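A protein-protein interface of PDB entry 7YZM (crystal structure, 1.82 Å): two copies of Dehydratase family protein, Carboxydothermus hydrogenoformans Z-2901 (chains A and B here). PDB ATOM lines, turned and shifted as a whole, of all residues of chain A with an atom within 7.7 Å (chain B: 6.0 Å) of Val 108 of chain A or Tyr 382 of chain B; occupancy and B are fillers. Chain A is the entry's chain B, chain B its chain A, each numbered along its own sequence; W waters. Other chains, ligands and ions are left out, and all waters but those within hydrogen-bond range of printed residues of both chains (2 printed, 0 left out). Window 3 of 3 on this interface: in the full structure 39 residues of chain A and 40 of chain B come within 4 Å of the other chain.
The side-chain amino group of Lys 149 of chain A lies within salt-bridge range of the side-chain carboxylate of Glu 380 of chain B. The guanidinium group (NH2) of Arg 386 of chain B is in salt-bridge range of the side-chain carboxylate (OE2) of Glu 156 of chain A (2.6 Å).
Val 108 of chain A touches just one residue of chain B: Tyr 382. Of chain A, only Val 108 and Ile 153 come within 4 Å of Tyr 382 of chain B. No residue of chain A comes within 4 Å of Ser 381 of chain B. Printed residues of chain A within 4 Å of Gly 378 of chain B: Pro 110. Of the printed residues of chain B, Glu 156 of chain A touches Leu 383 (3.4 Å) and Arg 386 (2.6 Å). Ala 150 of chain A touches none of the printed residues of chain B. The nearest residue of chain B that does not touch Val 108 of chain A is Val 379 of chain B (4.9 Å). The nearest printed residue of chain A that does not touch Gly 378 of chain B is Leu 109 of chain A (6.2 Å).
No position is printed for both chains. Of the 11 pairs that touch across the chains among the printed residues, none has its exchanged pair printed and touching as well.
Of the 11 printed residues of chain B, 6 touch a printed residue of chain A. Printed residues of chain B that touch a printed residue of chain A: Gly 378, Val 379, Glu 380, Tyr 382, Leu 383 and Arg 386. Of the 22 printed residues of chain A, 7 touch a printed residue of chain B. Hydrophobic or aromatic side chains of chain A that line the printed part of chain B: Val 108, Pro 110, Leu 113 and Ile 153. Among the printed residues, 11 pairs touch across the chains.
NZ of Lys 149 of chain A is in salt-bridge range of OE2 of Glu 152 of chain A. OG of Ser 381 of chain B is in hydrogen-bond range of O of Gly 378 of chain B, at 2.7 Å.
Water W1 lies within hydrogen-bond range of OH of Tyr 382 of chain B (2.6 Å), OH of Tyr 157 of chain A (2.7 Å) and OE1 of Glu 156 of chain A (2.8 Å). Water W2 lies within hydrogen-bond range of O of Val 108 of chain A (2.7 Å) and O of Val 379 of chain B (2.7 Å).
Among the printed residues, merely in contact across the chains: Lys 149 of chain A with Val 379 of chain B, Glu 156 of chain A with Leu 383 of chain B, Val 108 of chain A with Tyr 382 of chain B, Pro 110 of chain A with Val 379 of chain B, Pro 110 of chain A with Gly 378 of chain B, Glu 152 of chain A with Leu 383 of chain B, Leu 113 of chain A with Val 379 of chain B, Ile 153 of chain A with Tyr 382 of chain B and Ile 153 of chain A with Val 379 of chain B.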
ATOM      1  N   VAL A 102       2.679 -11.583  -6.289  1.00  0.00           N
ATOM      2  CA  VAL A 102       3.343 -10.660  -7.211  1.00  0.00           C
ATOM      3  C   VAL A 102       4.399 -11.372  -8.046  1.00  0.00           C
ATOM      4  O   VAL A 102       4.391 -11.214  -9.277  1.00  0.00           O
ATOM      5  CB  VAL A 102       3.907  -9.456  -6.439  1.00  0.00           C
ATOM      6  CG1 VAL A 102       4.874  -8.667  -7.314  1.00  0.00           C
ATOM      7  CG2 VAL A 102       2.771  -8.572  -5.953  1.00  0.00           C
ATOM      8  N   PRO A 103       5.322 -12.154  -7.469  1.00  0.00           N
ATOM      9  CA  PRO A 103       6.325 -12.830  -8.313  1.00  0.00           C
ATOM     10  C   PRO A 103       5.717 -13.715  -9.391  1.00  0.00           C
ATOM     11  O   PRO A 103       6.249 -13.784 -10.506  1.00  0.00           O
ATOM     12  CB  PRO A 103       7.145 -13.638  -7.293  1.00  0.00           C
ATOM     13  CG  PRO A 103       7.002 -12.848  -5.998  1.00  0.00           C
ATOM     14  CD  PRO A 103       5.569 -12.367  -6.030  1.00  0.00           C
ATOM     15  N   ALA A 104       4.607 -14.390  -9.096  1.00  0.00           N
ATOM     16  CA  ALA A 104       3.944 -15.184 -10.120  1.00  0.00           C
ATOM     17  C   ALA A 104       3.395 -14.305 -11.239  1.00  0.00           C
ATOM     18  O   ALA A 104       3.464 -14.671 -12.418  1.00  0.00           O
ATOM     19  CB  ALA A 104       2.833 -16.015  -9.489  1.00  0.00           C
ATOM     20  N   GLY A 105       2.842 -13.143 -10.901  1.00  0.00           N
ATOM     21  CA  GLY A 105       2.405 -12.237 -11.948  1.00  0.00           C
ATOM     22  C   GLY A 105       3.557 -11.750 -12.800  1.00  0.00           C
ATOM     23  O   GLY A 105       3.405 -11.558 -14.008  1.00  0.00           O
ATOM     24  N   GLU A 106       4.724 -11.560 -12.187  1.00  0.00           N
ATOM     25  CA  GLU A 106       5.899 -11.091 -12.903  1.00  0.00           C
ATOM     26  C   GLU A 106       6.467 -12.123 -13.865  1.00  0.00           C
ATOM     27  O   GLU A 106       7.368 -11.783 -14.633  1.00  0.00           O
ATOM     28  CB  GLU A 106       6.961 -10.658 -11.897  1.00  0.00           C
ATOM     29  CG  GLU A 106       6.536  -9.418 -11.130  1.00  0.00           C
ATOM     30  CD  GLU A 106       7.504  -9.012 -10.039  1.00  0.00           C
ATOM     31  OE1 GLU A 106       8.383  -9.822  -9.667  1.00  0.00           O
ATOM     32  OE2 GLU A 106       7.381  -7.868  -9.551  1.00  0.00           O
ATOM     33  N   THR A 107       5.969 -13.359 -13.870  1.00  0.00           N
ATOM     34  CA  THR A 107       6.418 -14.286 -14.904  1.00  0.00           C
ATOM     35  C   THR A 107       5.910 -13.870 -16.278  1.00  0.00           C
ATOM     36  O   THR A 107       6.513 -14.261 -17.290  1.00  0.00           O
ATOM     37  CB  THR A 107       5.978 -15.726 -14.601  1.00  0.00           C
ATOM     38  OG1 THR A 107       4.556 -15.864 -14.707  1.00  0.00           O
ATOM     39  CG2 THR A 107       6.443 -16.149 -13.204  1.00  0.00           C
ATOM     40  N   VAL A 108       4.828 -13.076 -16.328  1.00  0.00           N
ATOM     41  CA  VAL A 108       4.265 -12.659 -17.613  1.00  0.00           C
ATOM     42  C   VAL A 108       4.027 -11.155 -17.757  1.00  0.00           C
ATOM     43  O   VAL A 108       3.595 -10.658 -18.813  1.00  0.00           O
ATOM     44  CB  VAL A 108       2.942 -13.399 -17.881  1.00  0.00           C
ATOM     45  CG1 VAL A 108       3.096 -14.905 -17.844  1.00  0.00           C
ATOM     46  CG2 VAL A 108       1.858 -12.967 -16.871  1.00  0.00           C
ATOM     47  N   LEU A 109       4.303 -10.432 -16.671  1.00  0.00           N
ATOM     48  CA  LEU A 109       4.093  -8.990 -16.644  1.00  0.00           C
ATOM     49  C   LEU A 109       5.362  -8.268 -16.217  1.00  0.00           C
ATOM     50  O   LEU A 109       6.177  -8.840 -15.501  1.00  0.00           O
ATOM     51  CB  LEU A 109       2.957  -8.587 -15.689  1.00  0.00           C
ATOM     52  CG  LEU A 109       1.560  -9.084 -16.042  1.00  0.00           C
ATOM     53  CD1 LEU A 109       0.592  -8.824 -14.893  1.00  0.00           C
ATOM     54  CD2 LEU A 109       1.085  -8.417 -17.321  1.00  0.00           C
ATOM     55  N   PRO A 110       5.556  -7.007 -16.624  1.00  0.00           N
ATOM     56  CA  PRO A 110       6.736  -6.261 -16.151  1.00  0.00           C
ATOM     57  C   PRO A 110       6.739  -6.124 -14.631  1.00  0.00           C
ATOM     58  O   PRO A 110       5.693  -6.071 -13.985  1.00  0.00           O
ATOM     59  CB  PRO A 110       6.602  -4.890 -16.837  1.00  0.00           C
ATOM     60  CG  PRO A 110       5.604  -5.101 -17.972  1.00  0.00           C
ATOM     61  CD  PRO A 110       4.702  -6.208 -17.524  1.00  0.00           C
ATOM     62  N   ARG A 111       7.941  -6.059 -14.054  1.00  0.00           N
ATOM     63  CA  ARG A 111       8.038  -5.810 -12.618  1.00  0.00           C
ATOM     64  C   ARG A 111       7.669  -4.368 -12.283  1.00  0.00           C
ATOM     65  O   ARG A 111       7.125  -4.110 -11.201  1.00  0.00           O
ATOM     66  CB  ARG A 111       9.442  -6.167 -12.120  1.00  0.00           C
ATOM     67  CG  ARG A 111       9.834  -7.617 -12.444  1.00  0.00           C
ATOM     68  CD  ARG A 111      10.974  -8.147 -11.576  1.00  0.00           C
ATOM     69  NE  ARG A 111      12.092  -7.212 -11.555  1.00  0.00           N
ATOM     70  CZ  ARG A 111      12.730  -6.826 -10.456  1.00  0.00           C
ATOM     71  NH1 ARG A 111      13.722  -5.951 -10.543  1.00  0.00           N
ATOM     72  NH2 ARG A 111      12.380  -7.308  -9.272  1.00  0.00           N
ATOM     73  N   LEU A 113       5.148  -2.585 -12.869  1.00  0.00           N
ATOM     74  CA  LEU A 113       3.731  -2.483 -13.152  1.00  0.00           C
ATOM     75  C   LEU A 113       3.012  -2.403 -11.817  1.00  0.00           C
ATOM     76  O   LEU A 113       3.541  -2.827 -10.787  1.00  0.00           O
ATOM     77  CB  LEU A 113       3.233  -3.678 -13.976  1.00  0.00           C
ATOM     78  CG  LEU A 113       1.977  -3.390 -14.797  1.00  0.00           C
ATOM     79  CD1 LEU A 113       2.282  -2.475 -15.978  1.00  0.00           C
ATOM     80  CD2 LEU A 113       1.321  -4.665 -15.286  1.00  0.00           C
ATOM     81  N   LYS A 118      -0.253  -7.135 -11.004  1.00  0.00           N
ATOM     82  CA  LYS A 118       0.651  -8.274 -10.851  1.00  0.00           C
ATOM     83  C   LYS A 118       0.087  -9.296  -9.875  1.00  0.00           C
ATOM     84  O   LYS A 118       0.154 -10.508 -10.121  1.00  0.00           O
ATOM     85  CB  LYS A 118       2.022  -7.800 -10.383  1.00  0.00           C
ATOM     86  CG  LYS A 118       2.626  -6.741 -11.271  1.00  0.00           C
ATOM     87  CD  LYS A 118       4.076  -6.501 -10.929  1.00  0.00           C
ATOM     88  CE  LYS A 118       4.205  -5.741  -9.623  1.00  0.00           C
ATOM     89  NZ  LYS A 118       5.630  -5.570  -9.257  1.00  0.00           N
ATOM     90  N   MET A 121      -2.970 -11.217 -11.528  1.00  0.00           N
ATOM     91  CA  MET A 121      -2.462 -12.190 -12.492  1.00  0.00           C
ATOM     92  C   MET A 121      -1.831 -13.383 -11.782  1.00  0.00           C
ATOM     93  O   MET A 121      -2.087 -14.541 -12.132  1.00  0.00           O
ATOM     94  CB  MET A 121      -1.443 -11.527 -13.420  1.00  0.00           C
ATOM     95  CG  MET A 121      -0.909 -12.436 -14.522  1.00  0.00           C
ATOM     96  SD  MET A 121      -2.145 -12.759 -15.788  1.00  0.00           S
ATOM     97  CE  MET A 121      -2.098 -11.219 -16.718  1.00  0.00           C
ATOM     98  N   GLY A 122      -0.991 -13.112 -10.785  1.00  0.00           N
ATOM     99  CA  GLY A 122      -0.335 -14.190 -10.067  1.00  0.00           C
ATOM    100  C   GLY A 122      -1.296 -15.121  -9.358  1.00  0.00           C
ATOM    101  O   GLY A 122      -1.037 -16.326  -9.268  1.00  0.00           O
ATOM    102  N   ILE A 125      -2.478 -17.467 -12.172  1.00  0.00           N
ATOM    103  CA  ILE A 125      -1.399 -18.340 -12.632  1.00  0.00           C
ATOM    104  C   ILE A 125      -1.105 -19.422 -11.600  1.00  0.00           C
ATOM    105  O   ILE A 125      -0.974 -20.605 -11.937  1.00  0.00           O
ATOM    106  CB  ILE A 125      -0.140 -17.514 -12.951  1.00  0.00           C
ATOM    107  CG1 ILE A 125      -0.324 -16.762 -14.272  1.00  0.00           C
ATOM    108  CG2 ILE A 125       1.093 -18.419 -13.006  1.00  0.00           C
ATOM    109  CD1 ILE A 125       0.824 -15.827 -14.615  1.00  0.00           C
ATOM    110  N   LYS A 149      -3.571  -4.063 -21.341  1.00  0.00           N
ATOM    111  CA  LYS A 149      -2.675  -4.993 -22.014  1.00  0.00           C
ATOM    112  C   LYS A 149      -2.578  -6.322 -21.277  1.00  0.00           C
ATOM    113  O   LYS A 149      -2.334  -7.355 -21.907  1.00  0.00           O
ATOM    114  CB  LYS A 149      -1.298  -4.359 -22.173  1.00  0.00           C
ATOM    115  CG  LYS A 149      -1.314  -3.028 -22.929  1.00  0.00           C
ATOM    116  CD  LYS A 149      -2.041  -3.114 -24.266  1.00  0.00           C
ATOM    117  CE  LYS A 149      -1.140  -3.759 -25.316  1.00  0.00           C
ATOM    118  NZ  LYS A 149      -1.825  -3.970 -26.617  1.00  0.00           N
ATOM    119  N   ALA A 150      -2.781  -6.324 -19.961  1.00  0.00           N
ATOM    120  CA  ALA A 150      -2.773  -7.585 -19.227  1.00  0.00           C
ATOM    121  C   ALA A 150      -3.940  -8.480 -19.630  1.00  0.00           C
ATOM    122  O   ALA A 150      -3.815  -9.712 -19.565  1.00  0.00           O
ATOM    123  CB  ALA A 150      -2.805  -7.319 -17.723  1.00  0.00           C
ATOM    124  N   GLU A 152      -5.029  -9.188 -22.492  1.00  0.00           N
ATOM    125  CA  GLU A 152      -4.602 -10.013 -23.614  1.00  0.00           C
ATOM    126  C   GLU A 152      -3.852 -11.248 -23.134  1.00  0.00           C
ATOM    127  O   GLU A 152      -3.941 -12.310 -23.762  1.00  0.00           O
ATOM    128  CB  GLU A 152      -3.732  -9.182 -24.566  1.00  0.00           C
ATOM    129  CG  GLU A 152      -4.375  -7.857 -25.021  1.00  0.00           C
ATOM    130  CD  GLU A 152      -3.414  -6.936 -25.787  1.00  0.00           C
ATOM    131  OE1 GLU A 152      -2.212  -7.257 -25.886  1.00  0.00           O
ATOM    132  OE2 GLU A 152      -3.865  -5.871 -26.275  1.00  0.00           O
ATOM    133  N   ILE A 153      -3.120 -11.129 -22.025  1.00  0.00           N
ATOM    134  CA  ILE A 153      -2.391 -12.259 -21.468  1.00  0.00           C
ATOM    135  C   ILE A 153      -3.313 -13.144 -20.634  1.00  0.00           C
ATOM    136  O   ILE A 153      -3.233 -14.379 -20.702  1.00  0.00           O
ATOM    137  CB  ILE A 153      -1.199 -11.751 -20.635  1.00  0.00           C
ATOM    138  CG1 ILE A 153      -0.201 -11.000 -21.520  1.00  0.00           C
ATOM    139  CG2 ILE A 153      -0.524 -12.907 -19.908  1.00  0.00           C
ATOM    140  CD1 ILE A 153       0.796 -10.117 -20.743  1.00  0.00           C
ATOM    141  N   LEU A 154      -4.178 -12.532 -19.822  1.00  0.00           N
ATOM    142  CA  LEU A 154      -5.044 -13.297 -18.929  1.00  0.00           C
ATOM    143  C   LEU A 154      -6.010 -14.176 -19.712  1.00  0.00           C
ATOM    144  O   LEU A 154      -6.367 -15.268 -19.255  1.00  0.00           O
ATOM    145  CB  LEU A 154      -5.810 -12.347 -18.006  1.00  0.00           C
ATOM    146  CG  LEU A 154      -6.785 -12.958 -16.994  1.00  0.00           C
ATOM    147  CD1 LEU A 154      -6.040 -13.871 -16.028  1.00  0.00           C
ATOM    148  CD2 LEU A 154      -7.528 -11.849 -16.241  1.00  0.00           C
ATOM    149  N   GLU A 156      -5.484 -16.133 -21.904  1.00  0.00           N
ATOM    150  CA  GLU A 156      -4.916 -17.465 -22.102  1.00  0.00           C
ATOM    151  C   GLU A 156      -5.267 -18.412 -20.961  1.00  0.00           C
ATOM    152  O   GLU A 156      -5.135 -19.630 -21.122  1.00  0.00           O
ATOM    153  CB  GLU A 156      -3.394 -17.364 -22.252  1.00  0.00           C
ATOM    154  CG  GLU A 156      -2.946 -16.260 -23.210  1.00  0.00           C
ATOM    155  CD  GLU A 156      -1.461 -15.931 -23.121  1.00  0.00           C
ATOM    156  OE1 GLU A 156      -0.978 -15.552 -22.031  1.00  0.00           O
ATOM    157  OE2 GLU A 156      -0.776 -16.035 -24.157  1.00  0.00           O
ATOM    158  N   TYR A 157      -5.707 -17.875 -19.821  1.00  0.00           N
ATOM    159  CA  TYR A 157      -6.009 -18.656 -18.633  1.00  0.00           C
ATOM    160  C   TYR A 157      -7.491 -18.763 -18.323  1.00  0.00           C
ATOM    161  O   TYR A 157      -7.890 -19.708 -17.639  1.00  0.00           O
ATOM    162  CB  TYR A 157      -5.301 -18.037 -17.418  1.00  0.00           C
ATOM    163  CG  TYR A 157      -3.809 -17.938 -17.584  1.00  0.00           C
ATOM    164  CD1 TYR A 157      -3.232 -16.860 -18.241  1.00  0.00           C
ATOM    165  CD2 TYR A 157      -2.973 -18.925 -17.089  1.00  0.00           C
ATOM    166  CE1 TYR A 157      -1.864 -16.771 -18.399  1.00  0.00           C
ATOM    167  CE2 TYR A 157      -1.604 -18.844 -17.241  1.00  0.00           C
ATOM    168  CZ  TYR A 157      -1.051 -17.764 -17.898  1.00  0.00           C
ATOM    169  OH  TYR A 157       0.319 -17.683 -18.055  1.00  0.00           O
ATOM    170  N   TYR B 377       4.069  -0.857 -24.409  1.00  0.00           N
ATOM    171  CA  TYR B 377       5.023  -1.711 -25.118  1.00  0.00           C
ATOM    172  C   TYR B 377       5.738  -2.671 -24.178  1.00  0.00           C
ATOM    173  O   TYR B 377       6.100  -3.778 -24.588  1.00  0.00           O
ATOM    174  CB  TYR B 377       6.024  -0.837 -25.885  1.00  0.00           C
ATOM    175  CG  TYR B 377       5.366  -0.227 -27.103  1.00  0.00           C
ATOM    176  CD1 TYR B 377       5.357  -0.902 -28.319  1.00  0.00           C
ATOM    177  CD2 TYR B 377       4.701   0.995 -27.023  1.00  0.00           C
ATOM    178  CE1 TYR B 377       4.730  -0.373 -29.430  1.00  0.00           C
ATOM    179  CE2 TYR B 377       4.068   1.536 -28.136  1.00  0.00           C
ATOM    180  CZ  TYR B 377       4.087   0.839 -29.336  1.00  0.00           C
ATOM    181  OH  TYR B 377       3.465   1.352 -30.448  1.00  0.00           O
ATOM    182  N   GLY B 378       5.919  -2.289 -22.914  1.00  0.00           N
ATOM    183  CA  GLY B 378       6.527  -3.203 -21.961  1.00  0.00           C
ATOM    184  C   GLY B 378       5.696  -4.455 -21.753  1.00  0.00           C
ATOM    185  O   GLY B 378       6.219  -5.574 -21.779  1.00  0.00           O
ATOM    186  N   VAL B 379       4.384  -4.283 -21.543  1.00  0.00           N
ATOM    187  CA  VAL B 379       3.513  -5.434 -21.310  1.00  0.00           C
ATOM    188  C   VAL B 379       3.402  -6.281 -22.574  1.00  0.00           C
ATOM    189  O   VAL B 379       3.498  -7.515 -22.527  1.00  0.00           O
ATOM    190  CB  VAL B 379       2.124  -4.985 -20.821  1.00  0.00           C
ATOM    191  CG1 VAL B 379       1.162  -6.190 -20.778  1.00  0.00           C
ATOM    192  CG2 VAL B 379       2.195  -4.326 -19.446  1.00  0.00           C
ATOM    193  N   GLU B 380       3.183  -5.632 -23.724  1.00  0.00           N
ATOM    194  CA  GLU B 380       2.991  -6.361 -24.976  1.00  0.00           C
ATOM    195  C   GLU B 380       4.235  -7.132 -25.399  1.00  0.00           C
ATOM    196  O   GLU B 380       4.124  -8.073 -26.196  1.00  0.00           O
ATOM    197  CB  GLU B 380       2.565  -5.388 -26.089  1.00  0.00           C
ATOM    198  CG  GLU B 380       2.104  -6.075 -27.375  1.00  0.00           C
ATOM    199  CD  GLU B 380       1.476  -5.122 -28.401  1.00  0.00           C
ATOM    200  OE1 GLU B 380       0.373  -4.603 -28.142  1.00  0.00           O
ATOM    201  OE2 GLU B 380       2.066  -4.918 -29.485  1.00  0.00           O
ATOM    202  N   SER B 381       5.415  -6.779 -24.879  1.00  0.00           N
ATOM    203  CA  SER B 381       6.622  -7.493 -25.286  1.00  0.00           C
ATOM    204  C   SER B 381       6.561  -8.969 -24.922  1.00  0.00           C
ATOM    205  O   SER B 381       7.238  -9.781 -25.563  1.00  0.00           O
ATOM    206  CB  SER B 381       7.873  -6.853 -24.670  1.00  0.00           C
ATOM    207  OG  SER B 381       7.921  -6.990 -23.261  1.00  0.00           O
ATOM    208  N   TYR B 382       5.765  -9.336 -23.914  1.00  0.00           N
ATOM    209  CA  TYR B 382       5.658 -10.741 -23.531  1.00  0.00           C
ATOM    210  C   TYR B 382       5.070 -11.580 -24.662  1.00  0.00           C
ATOM    211  O   TYR B 382       5.633 -12.617 -25.041  1.00  0.00           O
ATOM    212  CB  TYR B 382       4.807 -10.879 -22.269  1.00  0.00           C
ATOM    213  CG  TYR B 382       4.464 -12.314 -21.951  1.00  0.00           C
ATOM    214  CD1 TYR B 382       5.402 -13.157 -21.369  1.00  0.00           C
ATOM    215  CD2 TYR B 382       3.212 -12.832 -22.250  1.00  0.00           C
ATOM    216  CE1 TYR B 382       5.092 -14.480 -21.086  1.00  0.00           C
ATOM    217  CE2 TYR B 382       2.892 -14.145 -21.966  1.00  0.00           C
ATOM    218  CZ  TYR B 382       3.838 -14.966 -21.392  1.00  0.00           C
ATOM    219  OH  TYR B 382       3.518 -16.279 -21.117  1.00  0.00           O
ATOM    220  N   LEU B 383       3.933 -11.148 -25.215  1.00  0.00           N
ATOM    221  CA  LEU B 383       3.300 -11.917 -26.280  1.00  0.00           C
ATOM    222  C   LEU B 383       4.120 -11.862 -27.559  1.00  0.00           C
ATOM    223  O   LEU B 383       4.173 -12.849 -28.303  1.00  0.00           O
ATOM    224  CB  LEU B 383       1.879 -11.414 -26.542  1.00  0.00           C
ATOM    225  CG  LEU B 383       0.844 -11.668 -25.443  1.00  0.00           C
ATOM    226  CD1 LEU B 383      -0.481 -10.996 -25.802  1.00  0.00           C
ATOM    227  CD2 LEU B 383       0.641 -13.147 -25.206  1.00  0.00           C
ATOM    228  N   VAL B 384       4.779 -10.734 -27.827  1.00  0.00           N
ATOM    229  CA  VAL B 384       5.637 -10.644 -29.006  1.00  0.00           C
ATOM    230  C   VAL B 384       6.782 -11.642 -28.899  1.00  0.00           C
ATOM    231  O   VAL B 384       7.040 -12.421 -29.821  1.00  0.00           O
ATOM    232  CB  VAL B 384       6.157  -9.204 -29.185  1.00  0.00           C
ATOM    233  CG1 VAL B 384       7.275  -9.150 -30.218  1.00  0.00           C
ATOM    234  CG2 VAL B 384       5.012  -8.272 -29.576  1.00  0.00           C
ATOM    235  N   GLY B 385       7.500 -11.623 -27.778  1.00  0.00           N
ATOM    236  CA  GLY B 385       8.623 -12.529 -27.631  1.00  0.00           C
ATOM    237  C   GLY B 385       8.196 -13.981 -27.677  1.00  0.00           C
ATOM    238  O   GLY B 385       8.894 -14.828 -28.242  1.00  0.00           O
ATOM    239  N   ARG B 386       7.035 -14.285 -27.100  1.00  0.00           N
ATOM    240  CA  ARG B 386       6.559 -15.666 -27.081  1.00  0.00           C
ATOM    241  C   ARG B 386       6.279 -16.174 -28.491  1.00  0.00           C
ATOM    242  O   ARG B 386       6.614 -17.317 -28.823  1.00  0.00           O
ATOM    243  CB  ARG B 386       5.307 -15.771 -26.212  1.00  0.00           C
ATOM    244  CG  ARG B 386       5.097 -17.135 -25.565  1.00  0.00           C
ATOM    245  CD  ARG B 386       3.745 -17.204 -24.855  1.00  0.00           C
ATOM    246  NE  ARG B 386       2.663 -16.668 -25.683  1.00  0.00           N
ATOM    247  CZ  ARG B 386       1.385 -17.005 -25.561  1.00  0.00           C
ATOM    248  NH1 ARG B 386       1.008 -17.882 -24.639  1.00  0.00           N
ATOM    249  NH2 ARG B 386       0.477 -16.463 -26.366  1.00  0.00           N
ATOM    250  N   GLU B 387       5.675 -15.342 -29.338  1.00  0.00           N
ATOM    251  CA  GLU B 387       5.419 -15.787 -30.701  1.00  0.00           C
ATOM    252  C   GLU B 387       6.714 -15.901 -31.497  1.00  0.00           C
ATOM    253  O   GLU B 387       6.887 -16.847 -32.273  1.00  0.00           O
ATOM    254  CB  GLU B 387       4.438 -14.849 -31.401  1.00  0.00           C
ATOM    255  CG  GLU B 387       4.165 -15.230 -32.873  1.00  0.00           C
ATOM    256  CD  GLU B 387       3.379 -16.533 -33.045  1.00  0.00           C
ATOM    257  OE1 GLU B 387       2.907 -17.104 -32.035  1.00  0.00           O
ATOM    258  OE2 GLU B 387       3.230 -16.987 -34.205  1.00  0.00           O
HETATM  259  O   HOH W   1       1.034 -16.782 -20.506  1.00  0.00           O
HETATM  260  O   HOH W   2       4.357  -8.381 -20.080  1.00  0.00           O
